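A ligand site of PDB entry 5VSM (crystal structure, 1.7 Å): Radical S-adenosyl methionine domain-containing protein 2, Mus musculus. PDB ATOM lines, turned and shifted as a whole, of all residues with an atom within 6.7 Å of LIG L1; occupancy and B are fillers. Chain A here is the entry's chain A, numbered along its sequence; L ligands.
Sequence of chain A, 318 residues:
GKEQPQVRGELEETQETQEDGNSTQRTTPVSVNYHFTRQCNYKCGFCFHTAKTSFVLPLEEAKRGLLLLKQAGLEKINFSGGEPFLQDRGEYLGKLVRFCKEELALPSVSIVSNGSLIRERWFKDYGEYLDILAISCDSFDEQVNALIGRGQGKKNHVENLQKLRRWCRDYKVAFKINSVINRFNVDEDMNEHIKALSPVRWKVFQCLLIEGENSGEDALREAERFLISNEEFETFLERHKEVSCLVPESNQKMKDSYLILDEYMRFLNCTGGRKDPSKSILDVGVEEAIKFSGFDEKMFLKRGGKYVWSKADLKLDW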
ATOM      1  N   ARG A  38     -14.201  -6.984 -30.123  1.00  0.00           N
ATOM      2  CA  ARG A  38     -13.325  -6.521 -29.055  1.00  0.00           C
ATOM      3  C   ARG A  38     -11.878  -6.376 -29.498  1.00  0.00           C
ATOM      4  O   ARG A  38     -11.035  -5.952 -28.702  1.00  0.00           O
ATOM      5  CB  ARG A  38     -13.418  -7.447 -27.846  1.00  0.00           C
ATOM      6  CG  ARG A  38     -14.706  -7.276 -27.037  1.00  0.00           C
ATOM      7  CD  ARG A  38     -14.687  -8.179 -25.816  1.00  0.00           C
ATOM      8  NE  ARG A  38     -15.833  -7.963 -24.939  1.00  0.00           N
ATOM      9  CZ  ARG A  38     -15.835  -7.145 -23.893  1.00  0.00           C
ATOM     10  NH1 ARG A  38     -14.743  -6.438 -23.585  1.00  0.00           N
ATOM     11  NH2 ARG A  38     -16.925  -7.031 -23.142  1.00  0.00           N
ATOM     12  N   GLN A  39     -11.555  -6.705 -30.747  1.00  0.00           N
ATOM     13  CA  GLN A  39     -10.182  -6.579 -31.207  1.00  0.00           C
ATOM     14  C   GLN A  39      -9.893  -5.147 -31.608  1.00  0.00           C
ATOM     15  O   GLN A  39     -10.775  -4.416 -32.087  1.00  0.00           O
ATOM     16  CB  GLN A  39      -9.912  -7.532 -32.376  1.00  0.00           C
ATOM     17  CG  GLN A  39      -9.785  -9.006 -31.975  1.00  0.00           C
ATOM     18  CD  GLN A  39      -8.619  -9.249 -31.033  1.00  0.00           C
ATOM     19  OE1 GLN A  39      -7.457  -9.206 -31.436  1.00  0.00           O
ATOM     20  NE2 GLN A  39      -8.924  -9.503 -29.754  1.00  0.00           N
ATOM     21  N   CYS A  40      -8.649  -4.736 -31.410  1.00  0.00           N
ATOM     22  CA  CYS A  40      -8.249  -3.366 -31.711  1.00  0.00           C
ATOM     23  C   CYS A  40      -6.770  -3.324 -32.031  1.00  0.00           C
ATOM     24  O   CYS A  40      -5.993  -4.158 -31.553  1.00  0.00           O
ATOM     25  CB  CYS A  40      -8.547  -2.416 -30.548  1.00  0.00           C
ATOM     26  SG  CYS A  40      -8.243  -0.705 -31.024  1.00  0.00           S
ATOM     27  N   ASN A  41      -6.372  -2.316 -32.827  1.00  0.00           N
ATOM     28  CA  ASN A  41      -4.984  -2.111 -33.177  1.00  0.00           C
ATOM     29  C   ASN A  41      -4.282  -1.078 -32.310  1.00  0.00           C
ATOM     30  O   ASN A  41      -3.049  -0.944 -32.406  1.00  0.00           O
ATOM     31  CB  ASN A  41      -4.840  -1.692 -34.658  1.00  0.00           C
ATOM     32  CG  ASN A  41      -5.468  -0.328 -34.943  1.00  0.00           C
ATOM     33  OD1 ASN A  41      -6.538  -0.010 -34.414  1.00  0.00           O
ATOM     34  ND2 ASN A  41      -4.804   0.479 -35.775  1.00  0.00           N
ATOM     35  N   TYR A  42      -5.018  -0.347 -31.466  1.00  0.00           N
ATOM     36  CA  TYR A  42      -4.441   0.640 -30.559  1.00  0.00           C
ATOM     37  C   TYR A  42      -4.230   0.032 -29.176  1.00  0.00           C
ATOM     38  O   TYR A  42      -4.626  -1.107 -28.906  1.00  0.00           O
ATOM     39  CB  TYR A  42      -5.339   1.884 -30.457  1.00  0.00           C
ATOM     40  CG  TYR A  42      -5.140   2.941 -31.531  1.00  0.00           C
ATOM     41  CD1 TYR A  42      -4.406   2.677 -32.696  1.00  0.00           C
ATOM     42  CD2 TYR A  42      -5.683   4.210 -31.368  1.00  0.00           C
ATOM     43  CE1 TYR A  42      -4.234   3.670 -33.667  1.00  0.00           C
ATOM     44  CE2 TYR A  42      -5.518   5.197 -32.336  1.00  0.00           C
ATOM     45  CZ  TYR A  42      -4.795   4.927 -33.473  1.00  0.00           C
ATOM     46  OH  TYR A  42      -4.619   5.909 -34.423  1.00  0.00           O
ATOM     47  N   LYS A  43      -3.660   0.821 -28.277  1.00  0.00           N
ATOM     48  CA  LYS A  43      -3.271   0.334 -26.950  1.00  0.00           C
ATOM     49  C   LYS A  43      -3.619   1.352 -25.862  1.00  0.00           C
ATOM     50  O   LYS A  43      -2.860   1.534 -24.909  1.00  0.00           O
ATOM     51  CB  LYS A  43      -1.780   0.039 -26.877  1.00  0.00           C
ATOM     52  CG  LYS A  43      -1.271  -0.995 -27.847  1.00  0.00           C
ATOM     53  CD  LYS A  43      -1.683  -2.394 -27.464  1.00  0.00           C
ATOM     54  CE  LYS A  43      -0.911  -3.410 -28.302  1.00  0.00           C
ATOM     55  NZ  LYS A  43      -1.667  -4.678 -28.476  1.00  0.00           N
ATOM     56  N   CYS A  44      -4.761   2.027 -25.999  1.00  0.00           N
ATOM     57  CA  CYS A  44      -5.095   3.089 -25.055  1.00  0.00           C
ATOM     58  C   CYS A  44      -5.074   2.558 -23.625  1.00  0.00           C
ATOM     59  O   CYS A  44      -5.724   1.564 -23.312  1.00  0.00           O
ATOM     60  CB  CYS A  44      -6.466   3.678 -25.391  1.00  0.00           C
ATOM     61  SG  CYS A  44      -6.607   4.236 -27.126  1.00  0.00           S
ATOM     62  N   GLY A  45      -4.282   3.211 -22.758  1.00  0.00           N
ATOM     63  CA  GLY A  45      -4.089   2.699 -21.412  1.00  0.00           C
ATOM     64  C   GLY A  45      -5.346   2.676 -20.579  1.00  0.00           C
ATOM     65  O   GLY A  45      -5.442   1.888 -19.625  1.00  0.00           O
ATOM     66  N   PHE A  46      -6.332   3.512 -20.908  1.00  0.00           N
ATOM     67  CA  PHE A  46      -7.584   3.586 -20.158  1.00  0.00           C
ATOM     68  C   PHE A  46      -8.716   2.768 -20.775  1.00  0.00           C
ATOM     69  O   PHE A  46      -9.809   2.765 -20.218  1.00  0.00           O
ATOM     70  CB  PHE A  46      -8.043   5.036 -20.042  1.00  0.00           C
ATOM     71  CG  PHE A  46      -8.037   5.783 -21.345  1.00  0.00           C
ATOM     72  CD1 PHE A  46      -8.969   5.472 -22.350  1.00  0.00           C
ATOM     73  CD2 PHE A  46      -7.133   6.804 -21.561  1.00  0.00           C
ATOM     74  CE1 PHE A  46      -8.965   6.152 -23.565  1.00  0.00           C
ATOM     75  CE2 PHE A  46      -7.124   7.496 -22.771  1.00  0.00           C
ATOM     76  CZ  PHE A  46      -8.047   7.163 -23.770  1.00  0.00           C
ATOM     77  N   CYS A  47      -8.477   2.081 -21.882  1.00  0.00           N
ATOM     78  CA  CYS A  47      -9.539   1.450 -22.671  1.00  0.00           C
ATOM     79  C   CYS A  47     -10.534   0.688 -21.793  1.00  0.00           C
ATOM     80  O   CYS A  47     -10.143  -0.198 -21.034  1.00  0.00           O
ATOM     81  CB  CYS A  47      -8.926   0.494 -23.697  1.00  0.00           C
ATOM     82  SG  CYS A  47     -10.209  -0.383 -24.641  1.00  0.00           S
ATOM     83  N   PHE A  48     -11.833   1.030 -21.876  1.00  0.00           N
ATOM     84  CA  PHE A  48     -12.799   0.369 -21.015  1.00  0.00           C
ATOM     85  C   PHE A  48     -13.628  -0.700 -21.723  1.00  0.00           C
ATOM     86  O   PHE A  48     -14.583  -1.211 -21.123  1.00  0.00           O
ATOM     87  CB  PHE A  48     -13.707   1.387 -20.302  1.00  0.00           C
ATOM     88  CG  PHE A  48     -14.651   2.175 -21.184  1.00  0.00           C
ATOM     89  CD1 PHE A  48     -15.544   3.057 -20.595  1.00  0.00           C
ATOM     90  CD2 PHE A  48     -14.659   2.060 -22.563  1.00  0.00           C
ATOM     91  CE1 PHE A  48     -16.433   3.808 -21.358  1.00  0.00           C
ATOM     92  CE2 PHE A  48     -15.530   2.801 -23.339  1.00  0.00           C
ATOM     93  CZ  PHE A  48     -16.425   3.677 -22.734  1.00  0.00           C
ATOM     94  N   HIS A  49     -13.262  -1.094 -22.938  1.00  0.00           N
ATOM     95  CA  HIS A  49     -13.910  -2.215 -23.624  1.00  0.00           C
ATOM     96  C   HIS A  49     -12.802  -2.987 -24.340  1.00  0.00           C
ATOM     97  O   HIS A  49     -12.523  -2.750 -25.512  1.00  0.00           O
ATOM     98  CB  HIS A  49     -14.992  -1.761 -24.586  1.00  0.00           C
ATOM     99  CG  HIS A  49     -16.019  -2.820 -24.857  1.00  0.00           C
ATOM    100  ND1 HIS A  49     -17.022  -3.113 -23.961  1.00  0.00           N
ATOM    101  CD2 HIS A  49     -16.168  -3.682 -25.885  1.00  0.00           C
ATOM    102  CE1 HIS A  49     -17.752  -4.108 -24.431  1.00  0.00           C
ATOM    103  NE2 HIS A  49     -17.260  -4.465 -25.602  1.00  0.00           N
ATOM    104  N   THR A  50     -12.188  -3.910 -23.597  1.00  0.00           N
ATOM    105  CA  THR A  50     -10.878  -4.466 -23.925  1.00  0.00           C
ATOM    106  C   THR A  50     -10.988  -5.764 -24.721  1.00  0.00           C
ATOM    107  O   THR A  50     -12.055  -6.342 -24.888  1.00  0.00           O
ATOM    108  CB  THR A  50     -10.082  -4.689 -22.637  1.00  0.00           C
ATOM    109  OG1 THR A  50     -10.755  -5.635 -21.793  1.00  0.00           O
ATOM    110  CG2 THR A  50      -9.927  -3.359 -21.903  1.00  0.00           C
ATOM    111  N   GLY A  81     -16.684  -0.875 -30.467  1.00  0.00           N
ATOM    112  CA  GLY A  81     -15.855  -2.034 -30.205  1.00  0.00           C
ATOM    113  C   GLY A  81     -14.971  -1.856 -28.987  1.00  0.00           C
ATOM    114  O   GLY A  81     -15.429  -1.315 -27.982  1.00  0.00           O
ATOM    115  N   GLY A  82     -13.701  -2.292 -29.045  1.00  0.00           N
ATOM    116  CA  GLY A  82     -13.046  -2.745 -30.268  1.00  0.00           C
ATOM    117  C   GLY A  82     -12.901  -1.659 -31.341  1.00  0.00           C
ATOM    118  O   GLY A  82     -13.483  -0.581 -31.249  1.00  0.00           O
ATOM    119  N   GLU A  83     -12.109  -1.931 -32.382  1.00  0.00           N
ATOM    120  CA  GLU A  83     -12.018  -1.008 -33.501  1.00  0.00           C
ATOM    121  C   GLU A  83     -12.932  -1.512 -34.612  1.00  0.00           C
ATOM    122  O   GLU A  83     -12.645  -2.574 -35.187  1.00  0.00           O
ATOM    123  CB  GLU A  83     -10.586  -0.901 -33.995  1.00  0.00           C
ATOM    124  CG  GLU A  83     -10.427  -0.051 -35.245  1.00  0.00           C
ATOM    125  CD  GLU A  83     -11.291   1.188 -35.245  1.00  0.00           C
ATOM    126  OE1 GLU A  83     -11.299   1.930 -34.245  1.00  0.00           O
ATOM    127  OE2 GLU A  83     -11.968   1.448 -36.262  1.00  0.00           O
ATOM    128  N   SER A 113     -14.873   5.330 -34.111  1.00  0.00           N
ATOM    129  CA  SER A 113     -13.664   4.668 -34.577  1.00  0.00           C
ATOM    130  C   SER A 113     -12.423   5.417 -34.121  1.00  0.00           C
ATOM    131  O   SER A 113     -12.451   6.638 -33.940  1.00  0.00           O
ATOM    132  CB  SER A 113     -13.702   4.563 -36.111  1.00  0.00           C
ATOM    133  OG  SER A 113     -12.453   4.112 -36.634  1.00  0.00           O
ATOM    134  N   ASN A 114     -11.303   4.687 -33.988  1.00  0.00           N
ATOM    135  CA  ASN A 114     -10.061   5.422 -33.802  1.00  0.00           C
ATOM    136  C   ASN A 114      -9.524   6.000 -35.108  1.00  0.00           C
ATOM    137  O   ASN A 114      -8.553   6.762 -35.076  1.00  0.00           O
ATOM    138  CB  ASN A 114      -8.999   4.565 -33.093  1.00  0.00           C
ATOM    139  CG  ASN A 114      -8.441   3.405 -33.945  1.00  0.00           C
ATOM    140  OD1 ASN A 114      -8.336   3.467 -35.172  1.00  0.00           O
ATOM    141  ND2 ASN A 114      -7.999   2.342 -33.245  1.00  0.00           N
ATOM    142  N   SER A 136     -12.304   9.174 -32.386  1.00  0.00           N
ATOM    143  CA  SER A 136     -11.786   9.367 -31.033  1.00  0.00           C
ATOM    144  C   SER A 136     -10.410  10.015 -31.092  1.00  0.00           C
ATOM    145  O   SER A 136      -9.483   9.461 -31.698  1.00  0.00           O
ATOM    146  CB  SER A 136     -11.726   8.036 -30.311  1.00  0.00           C
ATOM    147  OG  SER A 136     -13.039   7.551 -30.052  1.00  0.00           O
ATOM    148  N   GLY A 149      -1.266   5.725 -25.604  1.00  0.00           N
ATOM    149  CA  GLY A 149      -1.541   4.511 -26.340  1.00  0.00           C
ATOM    150  C   GLY A 149      -2.502   4.670 -27.483  1.00  0.00           C
ATOM    151  O   GLY A 149      -2.869   3.670 -28.110  1.00  0.00           O
ATOM    152  N   ARG A 150      -2.938   5.902 -27.760  1.00  0.00           N
ATOM    153  CA  ARG A 150      -3.866   6.205 -28.850  1.00  0.00           C
ATOM    154  C   ARG A 150      -3.027   6.319 -30.127  1.00  0.00           C
ATOM    155  O   ARG A 150      -2.788   7.394 -30.684  1.00  0.00           O
ATOM    156  CB  ARG A 150      -4.647   7.478 -28.535  1.00  0.00           C
ATOM    157  CG  ARG A 150      -5.695   7.887 -29.581  1.00  0.00           C
ATOM    158  CD  ARG A 150      -6.964   7.058 -29.489  1.00  0.00           C
ATOM    159  NE  ARG A 150      -7.817   7.460 -28.381  1.00  0.00           N
ATOM    160  CZ  ARG A 150      -9.002   6.912 -28.118  1.00  0.00           C
ATOM    161  NH1 ARG A 150      -9.455   5.929 -28.882  1.00  0.00           N
ATOM    162  NH2 ARG A 150      -9.733   7.340 -27.100  1.00  0.00           N
ATOM    163  N   VAL A 180     -11.580  11.424 -24.530  1.00  0.00           N
ATOM    164  CA  VAL A 180     -11.609  10.921 -23.160  1.00  0.00           C
ATOM    165  C   VAL A 180     -10.754  11.852 -22.317  1.00  0.00           C
ATOM    166  O   VAL A 180      -9.558  12.001 -22.574  1.00  0.00           O
ATOM    167  CB  VAL A 180     -11.087   9.465 -23.064  1.00  0.00           C
ATOM    168  CG1 VAL A 180     -11.076   9.027 -21.591  1.00  0.00           C
ATOM    169  CG2 VAL A 180     -11.949   8.539 -23.912  1.00  0.00           C
ATOM    170  N   ARG A 221      -6.179  -3.838 -19.083  1.00  0.00           N
ATOM    171  CA  ARG A 221      -5.767  -2.463 -18.863  1.00  0.00           C
ATOM    172  C   ARG A 221      -5.986  -2.134 -17.396  1.00  0.00           C
ATOM    173  O   ARG A 221      -6.887  -2.685 -16.752  1.00  0.00           O
ATOM    174  CB  ARG A 221      -6.544  -1.496 -19.770  1.00  0.00           C
ATOM    175  CG  ARG A 221      -6.415  -1.828 -21.258  1.00  0.00           C
ATOM    176  CD  ARG A 221      -5.049  -1.445 -21.822  1.00  0.00           C
ATOM    177  NE  ARG A 221      -4.654  -2.308 -22.935  1.00  0.00           N
ATOM    178  CZ  ARG A 221      -4.949  -2.124 -24.217  1.00  0.00           C
ATOM    179  NH1 ARG A 221      -4.507  -2.989 -25.114  1.00  0.00           N
ATOM    180  NH2 ARG A 221      -5.698  -1.082 -24.612  1.00  0.00           N
HETATM  181 FE1  LIG L   1      -8.907   0.526 -29.134  1.00  0.00          FE
HETATM  182 FE2  LIG L   1      -8.316   2.712 -27.751  1.00  0.00          FE
HETATM  183 FE3  LIG L   1      -9.850   0.806 -26.688  1.00  0.00          FE
HETATM  184 FE4  LIG L   1     -10.986   2.325 -28.771  1.00  0.00          FE
HETATM  185  S1  LIG L   1     -10.208   3.020 -26.603  1.00  0.00           S
HETATM  186  S2  LIG L   1     -10.926  -0.033 -28.457  1.00  0.00           S
HETATM  187  S3  LIG L   1      -8.908   2.732 -29.917  1.00  0.00           S
HETATM  188  S4  LIG L   1      -7.643   0.585 -27.284  1.00  0.00           S
HETATM  189  N1  LG2 L   2     -12.079   1.865 -30.814  1.00  0.00           N
HETATM  190  C1  LG2 L   2     -13.100   2.904 -31.023  1.00  0.00           C
HETATM  191  C2  LG2 L   2     -12.575   4.217 -30.487  1.00  0.00           C
HETATM  192  O1  LG2 L   2     -11.725   4.307 -29.619  1.00  0.00           O
HETATM  193  C3  LG2 L   2     -14.452   2.577 -30.370  1.00  0.00           C
HETATM  194  C4  LG2 L   2     -14.397   1.689 -29.125  1.00  0.00           C
HETATM  195  S1  LG2 L   2     -13.526   2.509 -27.763  1.00  0.00           S
HETATM  196  C5  LG2 L   2     -13.611   1.220 -26.474  1.00  0.00           C
HETATM  197  O2  LG2 L   2     -13.067   5.334 -30.984  1.00  0.00           O
HETATM  198  N1  LG3 L   3     -13.623   6.202 -20.213  1.00  0.00           N
HETATM  199  C1  LG3 L   3     -14.404   6.917 -20.997  1.00  0.00           C
HETATM  200  N2  LG3 L   3     -14.420   6.762 -22.310  1.00  0.00           N
HETATM  201  C2  LG3 L   3     -13.649   5.851 -22.884  1.00  0.00           C
HETATM  202  N3  LG3 L   3     -13.446   5.480 -24.171  1.00  0.00           N
HETATM  203  C3  LG3 L   3     -12.516   4.473 -24.187  1.00  0.00           C
HETATM  204  N4  LG3 L   3     -12.111   4.222 -22.954  1.00  0.00           N
HETATM  205  C4  LG3 L   3     -12.789   5.063 -22.101  1.00  0.00           C
HETATM  206  C5  LG3 L   3     -12.812   5.263 -20.716  1.00  0.00           C
HETATM  207  N5  LG3 L   3     -11.969   4.509 -19.899  1.00  0.00           N
HETATM  208  C6  LG3 L   3     -14.183   6.090 -25.286  1.00  0.00           C
HETATM  209  C7  LG3 L   3     -13.528   5.847 -26.665  1.00  0.00           C
HETATM  210  C8  LG3 L   3     -14.737   6.104 -27.615  1.00  0.00           C
HETATM  211  C9  LG3 L   3     -15.956   5.802 -26.718  1.00  0.00           C
HETATM  212  C10 LG3 L   3     -16.744   4.602 -27.267  1.00  0.00           C
HETATM  213  O1  LG3 L   3     -15.429   5.391 -25.436  1.00  0.00           O
HETATM  214  O2  LG3 L   3     -12.451   6.764 -26.861  1.00  0.00           O
HETATM  215  O3  LG3 L   3     -14.774   7.475 -28.019  1.00  0.00           O
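The side-chain sulfur (SG) of Cys 40 binds an iron atom (FE1) of LIG L1, 2.4 Å away. A sulfur (S4) of LIG L1 sits close to the backbone NH (N) of Cys 44. The side-chain sulfur (SG) of Cys 44 is bound to an iron atom (FE2) of LIG L1 (2.4 Å). The side-chain sulfur of Cys 47 binds an iron atom (FE3) of LIG L1 (2.4 Å). A sulfur (S3) of LIG L1 sits close to the guanidinium group (NH1) of Arg 150 (3.4 Å). The side-chain amide nitrogen of Asn 114 sits close to a sulfur (S3) of LIG L1. N of Gly 82 sits close to S2 of LIG L1, at 3.6 Å. S4 of LIG L1 sits close to NH2 of Arg 221, 3.7 Å away. The guanidinium group of Arg 150 sits close to an oxygen (O1) of LG2 L2 (2.9 Å). O of Gly 82 sits close to N1 of LG2 L2 (2.9 Å). The side-chain carboxylate (OE1) of Glu 83 lies close to a nitrogen (N1) of LG2 L2 (3.5 Å). OG of Ser 136 sits at hydrogen-bond distance from O2 of LG2 L2, at 2.4 Å. NH2 of Arg 150 lies within hydrogen-bond range of O2 of LG3 L3, 2.8 Å away. O of Phe 46 is in hydrogen-bond range of N5 of LG3 L3, 2.8 Å away. N of Phe 48 lies close to N4 of LG3 L3, at 3.4 Å. O3 of LG3 L3 sits at hydrogen-bond distance from OG of Ser 136.
An oxygen (O1) of LG2 L2 is bound to an iron atom (FE4) of LIG L1.
The side-chain amide nitrogen of Asn 114 sits close to the side-chain sulfur of Cys 40 (3.8 Å). N of Tyr 42 lies close to SG of Cys 40, at 3.3 Å. NE of Arg 150 lies close to SG of Cys 44 (3.7 Å). The backbone carbonyl oxygen (O) of Cys 44 sits at hydrogen-bond distance from the guanidinium group (NH2) of Arg 221, at 2.9 Å. The backbone NH (N) of Cys 44 sits at hydrogen-bond distance from the backbone carbonyl oxygen (O) of Gly 149, 3.3 Å away. The backbone carbonyl oxygen (O) of His 49 lies close to the side-chain sulfur (SG) of Cys 47. N of Asn 114 lies within hydrogen-bond range of OE1 of Glu 83, 2.8 Å away. The side-chain amide nitrogen (ND2) of Asn 114 lies within hydrogen-bond range of the side-chain amide oxygen (OD1) of Asn 41 (3.0 Å).
Residues that only touch LIG L1: Tyr 42. Within 4 Å of LIG L1: Cys 40, Tyr 42, Cys 44, Cys 47, Gly 82, Asn 114, Arg 150 and Arg 221.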
